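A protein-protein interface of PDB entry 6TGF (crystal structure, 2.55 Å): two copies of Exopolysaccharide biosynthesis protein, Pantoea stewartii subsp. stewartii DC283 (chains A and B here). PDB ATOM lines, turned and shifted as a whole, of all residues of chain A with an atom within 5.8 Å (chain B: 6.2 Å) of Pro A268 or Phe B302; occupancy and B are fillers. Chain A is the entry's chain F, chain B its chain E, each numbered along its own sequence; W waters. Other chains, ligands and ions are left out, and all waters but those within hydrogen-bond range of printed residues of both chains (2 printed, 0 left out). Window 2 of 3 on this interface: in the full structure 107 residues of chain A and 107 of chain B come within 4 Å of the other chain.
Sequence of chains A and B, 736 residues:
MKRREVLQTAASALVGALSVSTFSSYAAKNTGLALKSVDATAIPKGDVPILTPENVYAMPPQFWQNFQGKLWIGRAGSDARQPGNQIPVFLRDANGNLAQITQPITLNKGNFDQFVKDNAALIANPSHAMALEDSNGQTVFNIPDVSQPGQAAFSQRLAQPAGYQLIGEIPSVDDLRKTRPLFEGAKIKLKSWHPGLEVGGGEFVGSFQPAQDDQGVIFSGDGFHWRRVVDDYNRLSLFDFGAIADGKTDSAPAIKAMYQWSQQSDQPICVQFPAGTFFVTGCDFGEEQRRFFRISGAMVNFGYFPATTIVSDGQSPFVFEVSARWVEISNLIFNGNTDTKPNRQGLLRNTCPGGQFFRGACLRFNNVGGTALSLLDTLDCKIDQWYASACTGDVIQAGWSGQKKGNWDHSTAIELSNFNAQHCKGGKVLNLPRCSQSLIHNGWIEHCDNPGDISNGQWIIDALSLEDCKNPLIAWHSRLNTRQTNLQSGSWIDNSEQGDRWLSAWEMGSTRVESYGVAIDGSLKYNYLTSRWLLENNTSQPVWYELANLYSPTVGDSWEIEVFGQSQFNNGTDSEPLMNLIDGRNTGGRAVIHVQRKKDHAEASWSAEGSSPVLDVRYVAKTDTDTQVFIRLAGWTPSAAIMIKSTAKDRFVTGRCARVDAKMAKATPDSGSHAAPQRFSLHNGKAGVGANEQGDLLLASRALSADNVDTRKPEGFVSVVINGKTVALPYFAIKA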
ATOM      1  N   ASN A 234       2.637   9.284  23.847  1.00  0.00           N
ATOM      2  CA  ASN A 234       2.653  10.535  23.041  1.00  0.00           C
ATOM      3  C   ASN A 234       2.393  10.225  21.559  1.00  0.00           C
ATOM      4  O   ASN A 234       2.599  11.137  20.732  1.00  0.00           O
ATOM      5  CB  ASN A 234       3.967  11.298  23.229  1.00  0.00           C
ATOM      6  CG  ASN A 234       4.163  11.778  24.653  1.00  0.00           C
ATOM      7  OD1 ASN A 234       3.261  12.368  25.246  1.00  0.00           O
ATOM      8  ND2 ASN A 234       5.343  11.543  25.204  1.00  0.00           N
ATOM      9  N   SER A 262      -6.345  12.162  29.785  1.00  0.00           N
ATOM     10  CA  SER A 262      -5.073  12.915  29.946  1.00  0.00           C
ATOM     11  C   SER A 262      -5.028  13.604  31.316  1.00  0.00           C
ATOM     12  O   SER A 262      -3.942  13.621  31.931  1.00  0.00           O
ATOM     13  CB  SER A 262      -4.892  13.909  28.827  1.00  0.00           C
ATOM     14  OG  SER A 262      -5.900  14.909  28.865  1.00  0.00           O
ATOM     15  N   ASP A 266      -2.643  12.027  34.012  1.00  0.00           N
ATOM     16  CA  ASP A 266      -1.598  13.086  34.083  1.00  0.00           C
ATOM     17  C   ASP A 266      -0.662  12.958  32.872  1.00  0.00           C
ATOM     18  O   ASP A 266       0.563  13.116  33.053  1.00  0.00           O
ATOM     19  CB  ASP A 266      -0.840  13.016  35.414  1.00  0.00           C
ATOM     20  CG  ASP A 266      -0.003  14.244  35.733  1.00  0.00           C
ATOM     21  OD1 ASP A 266      -0.265  15.311  35.139  1.00  0.00           O
ATOM     22  OD2 ASP A 266       0.911  14.124  36.576  1.00  0.00           O
ATOM     23  N   GLN A 267      -1.220  12.688  31.686  1.00  0.00           N
ATOM     24  CA  GLN A 267      -0.468  12.568  30.407  1.00  0.00           C
ATOM     25  C   GLN A 267      -0.584  13.887  29.645  1.00  0.00           C
ATOM     26  O   GLN A 267      -1.688  14.377  29.418  1.00  0.00           O
ATOM     27  CB  GLN A 267      -0.986  11.389  29.581  1.00  0.00           C
ATOM     28  CG  GLN A 267      -0.544  10.030  30.113  1.00  0.00           C
ATOM     29  CD  GLN A 267       0.920   9.741  29.884  1.00  0.00           C
ATOM     30  OE1 GLN A 267       1.674  10.573  29.381  1.00  0.00           O
ATOM     31  NE2 GLN A 267       1.342   8.545  30.260  1.00  0.00           N
ATOM     32  N   PRO A 268       0.545  14.494  29.215  1.00  0.00           N
ATOM     33  CA  PRO A 268       0.541  15.872  28.727  1.00  0.00           C
ATOM     34  C   PRO A 268       0.085  16.054  27.269  1.00  0.00           C
ATOM     35  O   PRO A 268      -0.281  17.170  26.930  1.00  0.00           O
ATOM     36  CB  PRO A 268       2.014  16.272  28.880  1.00  0.00           C
ATOM     37  CG  PRO A 268       2.771  14.986  28.614  1.00  0.00           C
ATOM     38  CD  PRO A 268       1.884  13.884  29.158  1.00  0.00           C
ATOM     39  N   ILE A 269       0.113  14.990  26.454  1.00  0.00           N
ATOM     40  CA  ILE A 269      -0.245  15.047  25.002  1.00  0.00           C
ATOM     41  C   ILE A 269      -1.676  15.579  24.864  1.00  0.00           C
ATOM     42  O   ILE A 269      -1.952  16.261  23.861  1.00  0.00           O
ATOM     43  CB  ILE A 269      -0.073  13.688  24.290  1.00  0.00           C
ATOM     44  CG1 ILE A 269      -0.049  13.883  22.768  1.00  0.00           C
ATOM     45  CG2 ILE A 269      -1.131  12.688  24.742  1.00  0.00           C
ATOM     46  CD1 ILE A 269      -0.121  12.613  21.954  1.00  0.00           C
ATOM     47  N   CYS A 270      -2.551  15.264  25.825  1.00  0.00           N
ATOM     48  CA  CYS A 270      -3.912  15.849  25.939  1.00  0.00           C
ATOM     49  C   CYS A 270      -4.752  15.399  24.730  1.00  0.00           C
ATOM     50  O   CYS A 270      -4.777  14.178  24.471  1.00  0.00           O
ATOM     51  CB  CYS A 270      -3.786  17.362  26.078  1.00  0.00           C
ATOM     52  SG  CYS A 270      -5.231  18.156  26.828  1.00  0.00           S
ATOM     53  N   ARG A 294      -4.065  21.240  26.145  1.00  0.00           N
ATOM     54  CA  ARG A 294      -3.347  21.162  24.846  1.00  0.00           C
ATOM     55  C   ARG A 294      -4.270  20.500  23.819  1.00  0.00           C
ATOM     56  O   ARG A 294      -4.950  19.521  24.178  1.00  0.00           O
ATOM     57  CB  ARG A 294      -2.032  20.391  24.997  1.00  0.00           C
ATOM     58  CG  ARG A 294      -1.312  20.115  23.684  1.00  0.00           C
ATOM     59  CD  ARG A 294      -0.187  19.117  23.868  1.00  0.00           C
ATOM     60  NE  ARG A 294       0.463  18.741  22.617  1.00  0.00           N
ATOM     61  CZ  ARG A 294      -0.032  17.900  21.710  1.00  0.00           C
ATOM     62  NH1 ARG A 294      -1.215  17.331  21.884  1.00  0.00           N
ATOM     63  NH2 ARG A 294       0.664  17.635  20.617  1.00  0.00           N
ATOM     64  N   GLU A 328      -2.173  25.298  24.814  1.00  0.00           N
ATOM     65  CA  GLU A 328      -1.366  25.112  23.579  1.00  0.00           C
ATOM     66  C   GLU A 328      -2.274  24.548  22.481  1.00  0.00           C
ATOM     67  O   GLU A 328      -2.750  23.407  22.637  1.00  0.00           O
ATOM     68  CB  GLU A 328      -0.190  24.165  23.832  1.00  0.00           C
ATOM     69  CG  GLU A 328       0.719  24.593  24.972  1.00  0.00           C
ATOM     70  CD  GLU A 328       1.863  23.631  25.248  1.00  0.00           C
ATOM     71  OE1 GLU A 328       1.973  22.620  24.520  1.00  0.00           O
ATOM     72  OE2 GLU A 328       2.641  23.891  26.193  1.00  0.00           O
ATOM     73  N   ARG A 359      -0.271  29.562  23.731  1.00  0.00           N
ATOM     74  CA  ARG A 359       0.716  29.188  22.683  1.00  0.00           C
ATOM     75  C   ARG A 359      -0.036  28.714  21.434  1.00  0.00           C
ATOM     76  O   ARG A 359      -0.563  27.583  21.456  1.00  0.00           O
ATOM     77  CB  ARG A 359       1.652  28.094  23.202  1.00  0.00           C
ATOM     78  CG  ARG A 359       2.737  28.589  24.148  1.00  0.00           C
ATOM     79  CD  ARG A 359       4.033  28.928  23.444  1.00  0.00           C
ATOM     80  NE  ARG A 359       4.606  27.772  22.767  1.00  0.00           N
ATOM     81  CZ  ARG A 359       5.680  27.808  21.987  1.00  0.00           C
ATOM     82  NH1 ARG A 359       6.315  28.951  21.779  1.00  0.00           N
ATOM     83  NH2 ARG A 359       6.118  26.698  21.417  1.00  0.00           N
ATOM     84  N   ALA B 275       9.788  10.172  28.110  1.00  0.00           N
ATOM     85  CA  ALA B 275       8.943  10.973  29.028  1.00  0.00           C
ATOM     86  C   ALA B 275       8.998  10.360  30.433  1.00  0.00           C
ATOM     87  O   ALA B 275       9.018   9.114  30.531  1.00  0.00           O
ATOM     88  CB  ALA B 275       7.528  11.044  28.510  1.00  0.00           C
ATOM     89  N   ALA B 298      11.727  14.100  26.040  1.00  0.00           N
ATOM     90  CA  ALA B 298      10.618  13.609  25.187  1.00  0.00           C
ATOM     91  C   ALA B 298      10.295  14.651  24.110  1.00  0.00           C
ATOM     92  O   ALA B 298       9.873  15.770  24.474  1.00  0.00           O
ATOM     93  CB  ALA B 298       9.412  13.305  26.037  1.00  0.00           C
ATOM     94  N   VAL B 300       8.059  16.072  22.134  1.00  0.00           N
ATOM     95  CA  VAL B 300       6.616  16.411  21.934  1.00  0.00           C
ATOM     96  C   VAL B 300       6.474  17.932  22.060  1.00  0.00           C
ATOM     97  O   VAL B 300       6.947  18.479  23.078  1.00  0.00           O
ATOM     98  CB  VAL B 300       5.710  15.679  22.944  1.00  0.00           C
ATOM     99  CG1 VAL B 300       4.232  15.889  22.641  1.00  0.00           C
ATOM    100  CG2 VAL B 300       6.028  14.195  23.026  1.00  0.00           C
ATOM    101  N   ASN B 301       5.852  18.579  21.068  1.00  0.00           N
ATOM    102  CA  ASN B 301       5.715  20.058  20.984  1.00  0.00           C
ATOM    103  C   ASN B 301       4.924  20.563  22.198  1.00  0.00           C
ATOM    104  O   ASN B 301       3.682  20.438  22.191  1.00  0.00           O
ATOM    105  CB  ASN B 301       5.067  20.507  19.670  1.00  0.00           C
ATOM    106  CG  ASN B 301       3.603  20.128  19.561  1.00  0.00           C
ATOM    107  OD1 ASN B 301       3.269  18.958  19.397  1.00  0.00           O
ATOM    108  ND2 ASN B 301       2.723  21.111  19.658  1.00  0.00           N
ATOM    109  N   PHE B 302       5.623  21.097  23.204  1.00  0.00           N
ATOM    110  CA  PHE B 302       5.022  21.736  24.405  1.00  0.00           C
ATOM    111  C   PHE B 302       5.480  23.197  24.479  1.00  0.00           C
ATOM    112  O   PHE B 302       4.671  24.089  24.163  1.00  0.00           O
ATOM    113  CB  PHE B 302       5.349  20.931  25.666  1.00  0.00           C
ATOM    114  CG  PHE B 302       4.714  19.563  25.706  1.00  0.00           C
ATOM    115  CD1 PHE B 302       3.341  19.413  25.570  1.00  0.00           C
ATOM    116  CD2 PHE B 302       5.485  18.424  25.880  1.00  0.00           C
ATOM    117  CE1 PHE B 302       2.757  18.155  25.602  1.00  0.00           C
ATOM    118  CE2 PHE B 302       4.898  17.167  25.918  1.00  0.00           C
ATOM    119  CZ  PHE B 302       3.536  17.035  25.774  1.00  0.00           C
ATOM    120  N   GLY B 303       6.737  23.432  24.867  1.00  0.00           N
ATOM    121  CA  GLY B 303       7.303  24.784  25.029  1.00  0.00           C
ATOM    122  C   GLY B 303       7.176  25.285  26.457  1.00  0.00           C
ATOM    123  O   GLY B 303       8.045  26.076  26.876  1.00  0.00           O
ATOM    124  N   TYR B 304       6.134  24.849  27.176  1.00  0.00           N
ATOM    125  CA  TYR B 304       5.877  25.213  28.595  1.00  0.00           C
ATOM    126  C   TYR B 304       6.533  24.173  29.510  1.00  0.00           C
ATOM    127  O   TYR B 304       7.585  24.493  30.102  1.00  0.00           O
ATOM    128  CB  TYR B 304       4.377  25.373  28.865  1.00  0.00           C
ATOM    129  CG  TYR B 304       3.782  26.667  28.369  1.00  0.00           C
ATOM    130  CD1 TYR B 304       4.454  27.870  28.530  1.00  0.00           C
ATOM    131  CD2 TYR B 304       2.537  26.699  27.760  1.00  0.00           C
ATOM    132  CE1 TYR B 304       3.916  29.065  28.081  1.00  0.00           C
ATOM    133  CE2 TYR B 304       1.983  27.887  27.311  1.00  0.00           C
ATOM    134  CZ  TYR B 304       2.676  29.074  27.468  1.00  0.00           C
ATOM    135  OH  TYR B 304       2.142  30.250  27.026  1.00  0.00           O
ATOM    136  N   PHE B 305       5.945  22.976  29.613  1.00  0.00           N
ATOM    137  CA  PHE B 305       6.407  21.891  30.516  1.00  0.00           C
ATOM    138  C   PHE B 305       6.866  20.696  29.689  1.00  0.00           C
ATOM    139  O   PHE B 305       6.047  19.935  29.177  1.00  0.00           O
ATOM    140  CB  PHE B 305       5.314  21.537  31.527  1.00  0.00           C
ATOM    141  CG  PHE B 305       4.998  22.666  32.473  1.00  0.00           C
ATOM    142  CD1 PHE B 305       4.209  23.727  32.062  1.00  0.00           C
ATOM    143  CD2 PHE B 305       5.513  22.691  33.761  1.00  0.00           C
ATOM    144  CE1 PHE B 305       3.923  24.777  32.920  1.00  0.00           C
ATOM    145  CE2 PHE B 305       5.227  23.742  34.619  1.00  0.00           C
ATOM    146  CZ  PHE B 305       4.434  24.784  34.197  1.00  0.00           C
ATOM    147  N   PRO B 306       8.197  20.519  29.516  1.00  0.00           N
ATOM    148  CA  PRO B 306       8.751  19.282  28.966  1.00  0.00           C
ATOM    149  C   PRO B 306       8.215  18.037  29.686  1.00  0.00           C
ATOM    150  O   PRO B 306       7.970  18.109  30.879  1.00  0.00           O
ATOM    151  CB  PRO B 306      10.258  19.430  29.215  1.00  0.00           C
ATOM    152  CG  PRO B 306      10.493  20.925  29.212  1.00  0.00           C
ATOM    153  CD  PRO B 306       9.237  21.515  29.818  1.00  0.00           C
ATOM    154  N   ALA B 307       8.067  16.929  28.956  1.00  0.00           N
ATOM    155  CA  ALA B 307       7.543  15.643  29.474  1.00  0.00           C
ATOM    156  C   ALA B 307       8.663  14.839  30.151  1.00  0.00           C
ATOM    157  O   ALA B 307       8.390  13.688  30.544  1.00  0.00           O
ATOM    158  CB  ALA B 307       6.893  14.863  28.356  1.00  0.00           C
ATOM    159  N   CYS B 362      13.218  25.049  25.241  1.00  0.00           N
ATOM    160  CA  CYS B 362      12.203  24.452  26.152  1.00  0.00           C
ATOM    161  C   CYS B 362      12.905  23.855  27.377  1.00  0.00           C
ATOM    162  O   CYS B 362      12.891  22.617  27.527  1.00  0.00           O
ATOM    163  CB  CYS B 362      11.375  23.400  25.423  1.00  0.00           C
ATOM    164  SG  CYS B 362      10.621  24.027  23.901  1.00  0.00           S
ATOM    165  N   GLN B 385      12.871  29.900  24.868  1.00  0.00           N
ATOM    166  CA  GLN B 385      11.839  29.230  25.707  1.00  0.00           C
ATOM    167  C   GLN B 385      12.510  28.543  26.903  1.00  0.00           C
ATOM    168  O   GLN B 385      12.469  27.303  26.970  1.00  0.00           O
ATOM    169  CB  GLN B 385      11.030  28.234  24.872  1.00  0.00           C
ATOM    170  CG  GLN B 385      10.061  28.899  23.907  1.00  0.00           C
ATOM    171  CD  GLN B 385       9.436  27.908  22.954  1.00  0.00           C
ATOM    172  OE1 GLN B 385       8.533  27.154  23.313  1.00  0.00           O
ATOM    173  NE2 GLN B 385       9.912  27.908  21.719  1.00  0.00           N
HETATM  174  O   HOH W   1       0.022  22.216  20.871  1.00  0.00           O
HETATM  175  O   HOH W   2       3.709  25.163  21.767  1.00  0.00           O
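OD1 of Asn B301 is in hydrogen-bond range of NH2 of Arg A294, at 3.2 Å.
OE1 of Gln B385 lies within hydrogen-bond range of NH2 of Arg A359.
The side-chain carboxylate of Glu A328 lies close to the backbone carbonyl oxygen of Phe B302.
Water W2 bridges O of Phe B302 and NH2 of Arg A359.
Water W1 bridges the side-chain amide nitrogen of Asn B301 (3.2 Å) and the backbone carbonyl oxygen of Glu A328 (3.5 Å).
No position is printed for both chains.
Of the 11 pairs that touch across the chains among the printed residues, none has its exchanged pair printed and touching as well.
The backbone carbonyl oxygen (O) of Arg A294 is in hydrogen-bond range of the side-chain sulfur (SG) of Cys A270, at 3.0 Å.
The backbone NH (N) of Cys B362 lies within hydrogen-bond range of the backbone carbonyl oxygen (O) of Gln B385, at 2.9 Å.
ND2 of Asn A234 touches CB of Ala B275, at 3.99 Å.
Asn A234 touches Val B300 (CG to CG2, 3.5 Å).
Pro A268 touches Phe B302 (O to CE1, 3.5 Å).
Arg A294 touches Phe B302 (CD to CE1, 3.5 Å).
Glu A328 touches Asn B301.
Glu A328 touches Tyr B304.
Arg A359 touches Phe B302 (NE to O, 3.9 Å).
Tyr B304 touches Arg A359 (CE2 to CG, 3.3 Å).
Gln A267 touches none of the printed residues of chain B.
Pro A268 touches just one residue of chain B: Phe B302 (3.5 Å).
Printed residues of chain B within 4 Å of Arg A294: Asn B301 (3.2 Å) and Phe B302 (3.5 Å).
Printed residues of chain B within 4 Å of Glu A328: Asn B301, Phe B302 and Tyr B304.
Of the printed residues of chain B, Arg A359 touches Phe B302 (3.9 Å), Tyr B304 (3.3 Å) and Gln B385 (3.1 Å).
Of the printed residues of chain A, Ala B275 touches Asn A234.
Of the printed residues of chain A, Asn B301 touches Arg A294 (3.2 Å) and Glu A328 (3.6 Å).
Of chain A, only Pro A268, Arg A294, Glu A328 and Arg A359 come within 4 Å of Phe B302.
Of the 12 printed residues of chain B, 6 touch a printed residue of chain A.
Hydrophobic or aromatic side chains of chain B within 4 Å of the printed part of chain A: Ala B275, Val B300, Phe B302 and Tyr B304.
Of the 10 printed residues of chain A, 5 touch a printed residue of chain B.
Among the printed residues, 11 pairs touch across the chains.
Among the printed residues, no Asp or Glu carboxylate lies within 4 Å of a Lys or Arg side-chain nitrogen of the other chain.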
